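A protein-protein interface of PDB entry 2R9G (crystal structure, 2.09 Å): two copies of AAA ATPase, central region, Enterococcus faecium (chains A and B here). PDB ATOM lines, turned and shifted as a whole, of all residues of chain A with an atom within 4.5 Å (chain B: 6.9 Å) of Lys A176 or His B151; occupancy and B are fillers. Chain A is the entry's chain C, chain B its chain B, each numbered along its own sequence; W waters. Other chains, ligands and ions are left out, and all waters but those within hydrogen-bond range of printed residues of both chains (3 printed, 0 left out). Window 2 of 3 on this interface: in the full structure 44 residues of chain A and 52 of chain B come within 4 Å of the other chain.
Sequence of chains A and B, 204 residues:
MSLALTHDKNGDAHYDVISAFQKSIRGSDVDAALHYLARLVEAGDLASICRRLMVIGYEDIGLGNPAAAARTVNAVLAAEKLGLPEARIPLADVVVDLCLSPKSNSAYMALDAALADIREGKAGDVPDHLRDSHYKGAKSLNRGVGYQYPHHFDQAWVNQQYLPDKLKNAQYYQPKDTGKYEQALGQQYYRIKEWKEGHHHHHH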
ATOM      1  N   ARG A  26       4.336  26.577 -26.314  1.00  0.00           N
ATOM      2  CA  ARG A  26       3.427  25.904 -25.369  1.00  0.00           C
ATOM      3  C   ARG A  26       4.085  25.719 -23.995  1.00  0.00           C
ATOM      4  O   ARG A  26       3.440  25.890 -22.950  1.00  0.00           O
ATOM      5  CB  ARG A  26       2.984  24.557 -25.958  1.00  0.00           C
ATOM      6  CG  ARG A  26       2.038  23.713 -25.109  1.00  0.00           C
ATOM      7  CD  ARG A  26       1.923  22.299 -25.684  1.00  0.00           C
ATOM      8  NE  ARG A  26       1.221  22.227 -26.973  1.00  0.00           N
ATOM      9  CZ  ARG A  26       1.458  21.319 -27.920  1.00  0.00           C
ATOM     10  NH1 ARG A  26       0.753  21.333 -29.046  1.00  0.00           N
ATOM     11  NH2 ARG A  26       2.394  20.391 -27.752  1.00  0.00           N
ATOM     12  N   ASP A  60      -2.760  26.813 -27.735  1.00  0.00           N
ATOM     13  CA  ASP A  60      -2.056  26.715 -26.462  1.00  0.00           C
ATOM     14  C   ASP A  60      -2.213  27.926 -25.563  1.00  0.00           C
ATOM     15  O   ASP A  60      -2.111  27.803 -24.343  1.00  0.00           O
ATOM     16  CB  ASP A  60      -0.584  26.387 -26.713  1.00  0.00           C
ATOM     17  CG  ASP A  60      -0.407  25.007 -27.342  1.00  0.00           C
ATOM     18  OD1 ASP A  60      -0.984  24.034 -26.803  1.00  0.00           O
ATOM     19  OD2 ASP A  60       0.295  24.884 -28.370  1.00  0.00           O
ATOM     20  N   LYS A 103      -1.385  30.094 -20.425  1.00  0.00           N
ATOM     21  CA  LYS A 103      -1.692  29.048 -21.385  1.00  0.00           C
ATOM     22  C   LYS A 103      -3.042  28.421 -21.073  1.00  0.00           C
ATOM     23  O   LYS A 103      -3.351  28.134 -19.913  1.00  0.00           O
ATOM     24  CB  LYS A 103      -0.622  27.954 -21.372  1.00  0.00           C
ATOM     25  CG  LYS A 103       0.819  28.433 -21.507  1.00  0.00           C
ATOM     26  CD  LYS A 103       1.097  28.978 -22.893  1.00  0.00           C
ATOM     27  CE  LYS A 103       2.536  29.422 -23.023  1.00  0.00           C
ATOM     28  NZ  LYS A 103       2.887  30.508 -22.080  1.00  0.00           N
ATOM     29  N   SER A 104      -3.836  28.207 -22.117  1.00  0.00           N
ATOM     30  CA  SER A 104      -5.086  27.491 -21.995  1.00  0.00           C
ATOM     31  C   SER A 104      -5.401  26.721 -23.270  1.00  0.00           C
ATOM     32  O   SER A 104      -5.396  27.287 -24.375  1.00  0.00           O
ATOM     33  CB  SER A 104      -6.230  28.447 -21.675  1.00  0.00           C
ATOM     34  OG  SER A 104      -7.444  27.731 -21.598  1.00  0.00           O
ATOM     35  N   ASN A 105      -5.676  25.428 -23.106  1.00  0.00           N
ATOM     36  CA  ASN A 105      -6.143  24.607 -24.203  1.00  0.00           C
ATOM     37  C   ASN A 105      -7.616  24.224 -24.048  1.00  0.00           C
ATOM     38  O   ASN A 105      -8.142  23.436 -24.839  1.00  0.00           O
ATOM     39  CB  ASN A 105      -5.249  23.365 -24.370  1.00  0.00           C
ATOM     40  CG  ASN A 105      -5.368  22.367 -23.201  1.00  0.00           C
ATOM     41  OD1 ASN A 105      -5.820  22.699 -22.100  1.00  0.00           O
ATOM     42  ND2 ASN A 105      -4.924  21.140 -23.444  1.00  0.00           N
ATOM     43  N   SER A 106      -8.268  24.801 -23.032  1.00  0.00           N
ATOM     44  CA  SER A 106      -9.624  24.417 -22.614  1.00  0.00           C
ATOM     45  C   SER A 106     -10.661  24.444 -23.728  1.00  0.00           C
ATOM     46  O   SER A 106     -11.439  23.509 -23.855  1.00  0.00           O
ATOM     47  CB  SER A 106     -10.100  25.271 -21.436  1.00  0.00           C
ATOM     48  OG  SER A 106     -10.171  26.639 -21.798  1.00  0.00           O
ATOM     49  N   GLN A 174     -14.364  22.723 -19.433  1.00  0.00           N
ATOM     50  CA  GLN A 174     -13.890  22.883 -18.070  1.00  0.00           C
ATOM     51  C   GLN A 174     -12.930  24.062 -18.035  1.00  0.00           C
ATOM     52  O   GLN A 174     -11.789  23.963 -18.508  1.00  0.00           O
ATOM     53  CB  GLN A 174     -13.287  21.590 -17.497  1.00  0.00           C
ATOM     54  CG  GLN A 174     -12.988  20.503 -18.523  1.00  0.00           C
ATOM     55  CD  GLN A 174     -13.200  19.095 -17.974  1.00  0.00           C
ATOM     56  OE1 GLN A 174     -12.335  18.230 -18.110  1.00  0.00           O
ATOM     57  NE2 GLN A 174     -14.356  18.860 -17.357  1.00  0.00           N
ATOM     58  N   PRO A 175     -13.412  25.198 -17.501  1.00  0.00           N
ATOM     59  CA  PRO A 175     -12.665  26.449 -17.455  1.00  0.00           C
ATOM     60  C   PRO A 175     -11.396  26.354 -16.629  1.00  0.00           C
ATOM     61  O   PRO A 175     -11.315  25.567 -15.680  1.00  0.00           O
ATOM     62  CB  PRO A 175     -13.645  27.417 -16.798  1.00  0.00           C
ATOM     63  CG  PRO A 175     -14.626  26.576 -16.103  1.00  0.00           C
ATOM     64  CD  PRO A 175     -14.751  25.341 -16.906  1.00  0.00           C
ATOM     65  N   LYS A 176     -10.406  27.147 -17.011  1.00  0.00           N
ATOM     66  CA  LYS A 176      -9.136  27.169 -16.311  1.00  0.00           C
ATOM     67  C   LYS A 176      -8.930  28.541 -15.701  1.00  0.00           C
ATOM     68  O   LYS A 176      -9.659  29.481 -16.008  1.00  0.00           O
ATOM     69  CB  LYS A 176      -8.004  26.782 -17.262  1.00  0.00           C
ATOM     70  CG  LYS A 176      -8.097  25.330 -17.728  1.00  0.00           C
ATOM     71  CD  LYS A 176      -6.781  24.850 -18.303  1.00  0.00           C
ATOM     72  CE  LYS A 176      -6.658  23.337 -18.213  1.00  0.00           C
ATOM     73  NZ  LYS A 176      -5.231  22.913 -18.349  1.00  0.00           N
ATOM     74  N   ASP A 177      -7.958  28.648 -14.808  1.00  0.00           N
ATOM     75  CA  ASP A 177      -7.719  29.907 -14.110  1.00  0.00           C
ATOM     76  C   ASP A 177      -6.267  30.353 -14.236  1.00  0.00           C
ATOM     77  O   ASP A 177      -5.739  31.039 -13.357  1.00  0.00           O
ATOM     78  CB  ASP A 177      -8.175  29.823 -12.637  1.00  0.00           C
ATOM     79  CG  ASP A 177      -7.561  28.644 -11.870  1.00  0.00           C
ATOM     80  OD1 ASP A 177      -6.489  28.120 -12.253  1.00  0.00           O
ATOM     81  OD2 ASP A 177      -8.167  28.244 -10.853  1.00  0.00           O
ATOM     82  N   THR A 178      -5.632  29.953 -15.340  1.00  0.00           N
ATOM     83  CA  THR A 178      -4.235  30.291 -15.606  1.00  0.00           C
ATOM     84  C   THR A 178      -4.058  31.786 -15.885  1.00  0.00           C
ATOM     85  O   THR A 178      -2.990  32.340 -15.641  1.00  0.00           O
ATOM     86  CB  THR A 178      -3.623  29.440 -16.754  1.00  0.00           C
ATOM     87  OG1 THR A 178      -4.525  29.401 -17.860  1.00  0.00           O
ATOM     88  CG2 THR A 178      -3.362  28.018 -16.297  1.00  0.00           C
ATOM     89  N   GLU A 182      -9.893  34.160 -18.235  1.00  0.00           N
ATOM     90  CA  GLU A 182     -10.641  32.911 -18.144  1.00  0.00           C
ATOM     91  C   GLU A 182     -11.077  32.594 -16.705  1.00  0.00           C
ATOM     92  O   GLU A 182     -11.957  31.757 -16.489  1.00  0.00           O
ATOM     93  CB  GLU A 182      -9.844  31.756 -18.748  1.00  0.00           C
ATOM     94  CG  GLU A 182     -10.705  30.646 -19.330  1.00  0.00           C
ATOM     95  CD  GLU A 182      -9.921  29.389 -19.686  1.00  0.00           C
ATOM     96  OE1 GLU A 182      -8.674  29.391 -19.600  1.00  0.00           O
ATOM     97  OE2 GLU A 182     -10.563  28.390 -20.051  1.00  0.00           O
ATOM     98  N   GLN A 183     -10.464  33.266 -15.730  1.00  0.00           N
ATOM     99  CA  GLN A 183     -10.945  33.231 -14.350  1.00  0.00           C
ATOM    100  C   GLN A 183     -12.366  33.784 -14.327  1.00  0.00           C
ATOM    101  O   GLN A 183     -13.263  33.181 -13.750  1.00  0.00           O
ATOM    102  CB  GLN A 183     -10.067  34.084 -13.439  1.00  0.00           C
ATOM    103  CG  GLN A 183      -8.754  33.463 -13.035  1.00  0.00           C
ATOM    104  CD  GLN A 183      -7.895  34.414 -12.218  1.00  0.00           C
ATOM    105  OE1 GLN A 183      -8.400  35.367 -11.620  1.00  0.00           O
ATOM    106  NE2 GLN A 183      -6.587  34.162 -12.193  1.00  0.00           N
ATOM    107  N   TYR B 147       7.872  13.095 -24.004  1.00  0.00           N
ATOM    108  CA  TYR B 147       7.332  14.457 -24.068  1.00  0.00           C
ATOM    109  C   TYR B 147       6.237  14.696 -23.021  1.00  0.00           C
ATOM    110  O   TYR B 147       5.303  13.896 -22.890  1.00  0.00           O
ATOM    111  CB  TYR B 147       6.816  14.788 -25.485  1.00  0.00           C
ATOM    112  CG  TYR B 147       6.105  16.124 -25.555  1.00  0.00           C
ATOM    113  CD1 TYR B 147       6.802  17.320 -25.331  1.00  0.00           C
ATOM    114  CD2 TYR B 147       4.739  16.197 -25.807  1.00  0.00           C
ATOM    115  CE1 TYR B 147       6.156  18.545 -25.361  1.00  0.00           C
ATOM    116  CE2 TYR B 147       4.081  17.421 -25.845  1.00  0.00           C
ATOM    117  CZ  TYR B 147       4.797  18.589 -25.619  1.00  0.00           C
ATOM    118  OH  TYR B 147       4.149  19.803 -25.658  1.00  0.00           O
ATOM    119  N   GLN B 148       6.381  15.782 -22.262  1.00  0.00           N
ATOM    120  CA  GLN B 148       5.387  16.168 -21.262  1.00  0.00           C
ATOM    121  C   GLN B 148       4.616  17.400 -21.713  1.00  0.00           C
ATOM    122  O   GLN B 148       5.201  18.444 -22.007  1.00  0.00           O
ATOM    123  CB  GLN B 148       6.038  16.430 -19.903  1.00  0.00           C
ATOM    124  CG  GLN B 148       6.958  15.322 -19.407  1.00  0.00           C
ATOM    125  CD  GLN B 148       7.646  15.704 -18.114  1.00  0.00           C
ATOM    126  OE1 GLN B 148       7.080  15.541 -17.032  1.00  0.00           O
ATOM    127  NE2 GLN B 148       8.872  16.228 -18.218  1.00  0.00           N
ATOM    128  N   TYR B 149       3.297  17.255 -21.744  1.00  0.00           N
ATOM    129  CA  TYR B 149       2.363  18.242 -22.275  1.00  0.00           C
ATOM    130  C   TYR B 149       2.002  19.197 -21.140  1.00  0.00           C
ATOM    131  O   TYR B 149       1.323  18.787 -20.196  1.00  0.00           O
ATOM    132  CB  TYR B 149       1.136  17.476 -22.779  1.00  0.00           C
ATOM    133  CG  TYR B 149       0.038  18.242 -23.485  1.00  0.00           C
ATOM    134  CD1 TYR B 149       0.246  18.826 -24.734  1.00  0.00           C
ATOM    135  CD2 TYR B 149      -1.244  18.307 -22.934  1.00  0.00           C
ATOM    136  CE1 TYR B 149      -0.796  19.501 -25.401  1.00  0.00           C
ATOM    137  CE2 TYR B 149      -2.289  18.969 -23.588  1.00  0.00           C
ATOM    138  CZ  TYR B 149      -2.058  19.564 -24.815  1.00  0.00           C
ATOM    139  OH  TYR B 149      -3.091  20.216 -25.448  1.00  0.00           O
ATOM    140  N   PRO B 150       2.472  20.462 -21.214  1.00  0.00           N
ATOM    141  CA  PRO B 150       2.399  21.439 -20.109  1.00  0.00           C
ATOM    142  C   PRO B 150       0.999  21.684 -19.548  1.00  0.00           C
ATOM    143  O   PRO B 150       0.874  22.001 -18.370  1.00  0.00           O
ATOM    144  CB  PRO B 150       2.949  22.724 -20.739  1.00  0.00           C
ATOM    145  CG  PRO B 150       3.813  22.261 -21.832  1.00  0.00           C
ATOM    146  CD  PRO B 150       3.126  21.048 -22.395  1.00  0.00           C
ATOM    147  N   HIS B 151      -0.033  21.502 -20.374  1.00  0.00           N
ATOM    148  CA  HIS B 151      -1.427  21.729 -19.976  1.00  0.00           C
ATOM    149  C   HIS B 151      -1.973  20.754 -18.918  1.00  0.00           C
ATOM    150  O   HIS B 151      -3.021  21.008 -18.324  1.00  0.00           O
ATOM    151  CB  HIS B 151      -2.346  21.717 -21.202  1.00  0.00           C
ATOM    152  CG  HIS B 151      -2.030  22.774 -22.218  1.00  0.00           C
ATOM    153  ND1 HIS B 151      -2.253  24.115 -21.994  1.00  0.00           N
ATOM    154  CD2 HIS B 151      -1.528  22.681 -23.471  1.00  0.00           C
ATOM    155  CE1 HIS B 151      -1.892  24.804 -23.061  1.00  0.00           C
ATOM    156  NE2 HIS B 151      -1.448  23.957 -23.973  1.00  0.00           N
ATOM    157  N   HIS B 152      -1.270  19.646 -18.683  1.00  0.00           N
ATOM    158  CA  HIS B 152      -1.659  18.691 -17.642  1.00  0.00           C
ATOM    159  C   HIS B 152      -1.150  19.126 -16.279  1.00  0.00           C
ATOM    160  O   HIS B 152      -1.599  18.616 -15.252  1.00  0.00           O
ATOM    161  CB  HIS B 152      -1.104  17.301 -17.932  1.00  0.00           C
ATOM    162  CG  HIS B 152      -1.659  16.668 -19.167  1.00  0.00           C
ATOM    163  ND1 HIS B 152      -0.887  15.906 -20.016  1.00  0.00           N
ATOM    164  CD2 HIS B 152      -2.906  16.674 -19.693  1.00  0.00           C
ATOM    165  CE1 HIS B 152      -1.636  15.464 -21.010  1.00  0.00           C
ATOM    166  NE2 HIS B 152      -2.864  15.923 -20.842  1.00  0.00           N
ATOM    167  N   PHE B 153      -0.207  20.065 -16.283  1.00  0.00           N
ATOM    168  CA  PHE B 153       0.504  20.474 -15.081  1.00  0.00           C
ATOM    169  C   PHE B 153      -0.089  21.725 -14.435  1.00  0.00           C
ATOM    170  O   PHE B 153      -0.873  22.449 -15.056  1.00  0.00           O
ATOM    171  CB  PHE B 153       1.988  20.698 -15.397  1.00  0.00           C
ATOM    172  CG  PHE B 153       2.735  19.440 -15.725  1.00  0.00           C
ATOM    173  CD1 PHE B 153       2.638  18.864 -16.992  1.00  0.00           C
ATOM    174  CD2 PHE B 153       3.541  18.830 -14.770  1.00  0.00           C
ATOM    175  CE1 PHE B 153       3.315  17.690 -17.292  1.00  0.00           C
ATOM    176  CE2 PHE B 153       4.231  17.656 -15.064  1.00  0.00           C
ATOM    177  CZ  PHE B 153       4.117  17.084 -16.325  1.00  0.00           C
ATOM    178  N   ASP B 154       0.288  21.951 -13.178  1.00  0.00           N
ATOM    179  CA  ASP B 154      -0.061  23.163 -12.447  1.00  0.00           C
ATOM    180  C   ASP B 154       0.601  24.363 -13.116  1.00  0.00           C
ATOM    181  O   ASP B 154       1.731  24.261 -13.600  1.00  0.00           O
ATOM    182  CB  ASP B 154       0.394  23.055 -10.987  1.00  0.00           C
ATOM    183  CG  ASP B 154      -0.198  24.142 -10.105  1.00  0.00           C
ATOM    184  OD1 ASP B 154      -1.442  24.210  -9.989  1.00  0.00           O
ATOM    185  OD2 ASP B 154       0.584  24.926  -9.522  1.00  0.00           O
ATOM    186  N   ALA B 156      -0.044  25.449 -15.888  1.00  0.00           N
ATOM    187  CA  ALA B 156       0.189  25.009 -17.276  1.00  0.00           C
ATOM    188  C   ALA B 156       1.668  25.070 -17.702  1.00  0.00           C
ATOM    189  O   ALA B 156       1.999  25.576 -18.781  1.00  0.00           O
ATOM    190  CB  ALA B 156      -0.716  25.760 -18.265  1.00  0.00           C
ATOM    191  N   TRP B 157       2.539  24.552 -16.836  1.00  0.00           N
ATOM    192  CA  TRP B 157       3.978  24.587 -17.052  1.00  0.00           C
ATOM    193  C   TRP B 157       4.651  23.328 -16.520  1.00  0.00           C
ATOM    194  O   TRP B 157       4.374  22.891 -15.407  1.00  0.00           O
ATOM    195  CB  TRP B 157       4.598  25.821 -16.383  1.00  0.00           C
ATOM    196  CG  TRP B 157       6.090  25.915 -16.588  1.00  0.00           C
ATOM    197  CD1 TRP B 157       6.735  26.447 -17.667  1.00  0.00           C
ATOM    198  CD2 TRP B 157       7.117  25.445 -15.699  1.00  0.00           C
ATOM    199  NE1 TRP B 157       8.094  26.340 -17.507  1.00  0.00           N
ATOM    200  CE2 TRP B 157       8.356  25.731 -16.308  1.00  0.00           C
ATOM    201  CE3 TRP B 157       7.109  24.812 -14.446  1.00  0.00           C
ATOM    202  CZ2 TRP B 157       9.578  25.412 -15.706  1.00  0.00           C
ATOM    203  CZ3 TRP B 157       8.328  24.495 -13.849  1.00  0.00           C
ATOM    204  CH2 TRP B 157       9.542  24.797 -14.478  1.00  0.00           C
ATOM    205  N   VAL B 158       5.549  22.767 -17.322  1.00  0.00           N
ATOM    206  CA  VAL B 158       6.390  21.655 -16.897  1.00  0.00           C
ATOM    207  C   VAL B 158       7.866  22.033 -17.069  1.00  0.00           C
ATOM    208  O   VAL B 158       8.231  22.714 -18.037  1.00  0.00           O
ATOM    209  CB  VAL B 158       6.033  20.334 -17.662  1.00  0.00           C
ATOM    210  CG1 VAL B 158       6.042  20.527 -19.193  1.00  0.00           C
ATOM    211  CG2 VAL B 158       6.940  19.167 -17.238  1.00  0.00           C
HETATM  212  O   HOH W   1      -3.671  25.046 -19.830  1.00  0.00           O
HETATM  213  O   HOH W   2      -2.347  21.880 -27.161  1.00  0.00           O
HETATM  214  O   HOH W   3       3.998  26.378 -20.249  1.00  0.00           O
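The side-chain hydroxyl of Tyr B147 is in hydrogen-bond range of the guanidinium group of Arg A26, 2.8 Å away.
ND2 of Asn A105 sits at hydrogen-bond distance from OH of Tyr B149.
The side-chain carboxylate of Asp A60 is in hydrogen-bond range of a ring nitrogen (NE2) of His B151.
O of His B151 sits at hydrogen-bond distance from NZ of Lys A176 (2.9 Å).
O of Pro B150 lies within hydrogen-bond range of N of Trp B157, 3.4 Å away.
NE of Arg A26 is in salt-bridge range of OD1 of Asp A60.
The backbone carbonyl oxygen of Asp A60 is in hydrogen-bond range of the backbone NH of Ser A104, at 2.8 Å.
The backbone carbonyl oxygen (O) of Lys A103 sits at hydrogen-bond distance from the side-chain hydroxyl (OG1) of Thr A178, 2.7 Å away.
OE2 of Glu A182 is in hydrogen-bond range of N of Lys A176 (3.3 Å).
Among the printed residues, pairs that only touch across the chains: Arg A26 with Tyr B149 (3.7 Å), Arg A26 with Pro B150 (3.7 Å), Arg A26 with His B151 (3.7 Å), Lys A103 with His B151 (3.8 Å), Lys A103 with Ala B156 (3.8 Å), Asn A105 with His B151 (3.5 Å) and Thr A178 with Ala B156 (3.997 Å).
Printed residues of chain B within 4 Å of Asn A105: Tyr B149 (2.9 Å) and His B151 (3.5 Å).
Of chain B, only His B151 comes within 4 Å of Lys A176.
Printed residues of chain A within 4 Å of Tyr B147: Arg A26 (2.8 Å).
Of the printed residues of chain A, Tyr B149 touches Arg A26 (3.7 Å) and Asn A105 (2.9 Å).
Printed residues of chain A within 4 Å of Pro B150: Arg A26 (3.7 Å).
Printed residues of chain A within 4 Å of His B151: Arg A26 (3.7 Å), Asp A60 (2.9 Å), Lys A103 (3.8 Å), Asn A105 (3.5 Å) and Lys A176 (2.9 Å).
Of the printed residues of chain A, Ala B156 touches Lys A103 (3.8 Å) and Thr A178 (3.997 Å).
The nearest printed residue of chain A that does not touch His B151 is Ser A104 (4.004 Å).
Along chain A the printed residues that touch a printed residue of chain B span positions 26 to 178.
Hydrophobic or aromatic side chains of chain B within 4 Å of the printed part of chain A: Tyr B147, Tyr B149, Pro B150, His B151 and Ala B156.
Among the printed residues, 11 pairs touch across the chains.
Among the printed residues, no Asp or Glu carboxylate lies within 4 Å of a Lys or Arg side-chain nitrogen of the other chain.
No position is printed for both chains.
Water W2 bridges the side-chain hydroxyl (OH) of Tyr B149 and the side-chain carboxylate (OD1) of Asp A60.
Water W3 lies within hydrogen-bond range of the backbone carbonyl oxygen of Ala B156 (2.6 Å) and the backbone carbonyl oxygen of Arg A26 (2.8 Å).
Water W1 lies within hydrogen-bond range of ND1 of His B151, NZ of Lys A176 and O of Lys A103.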
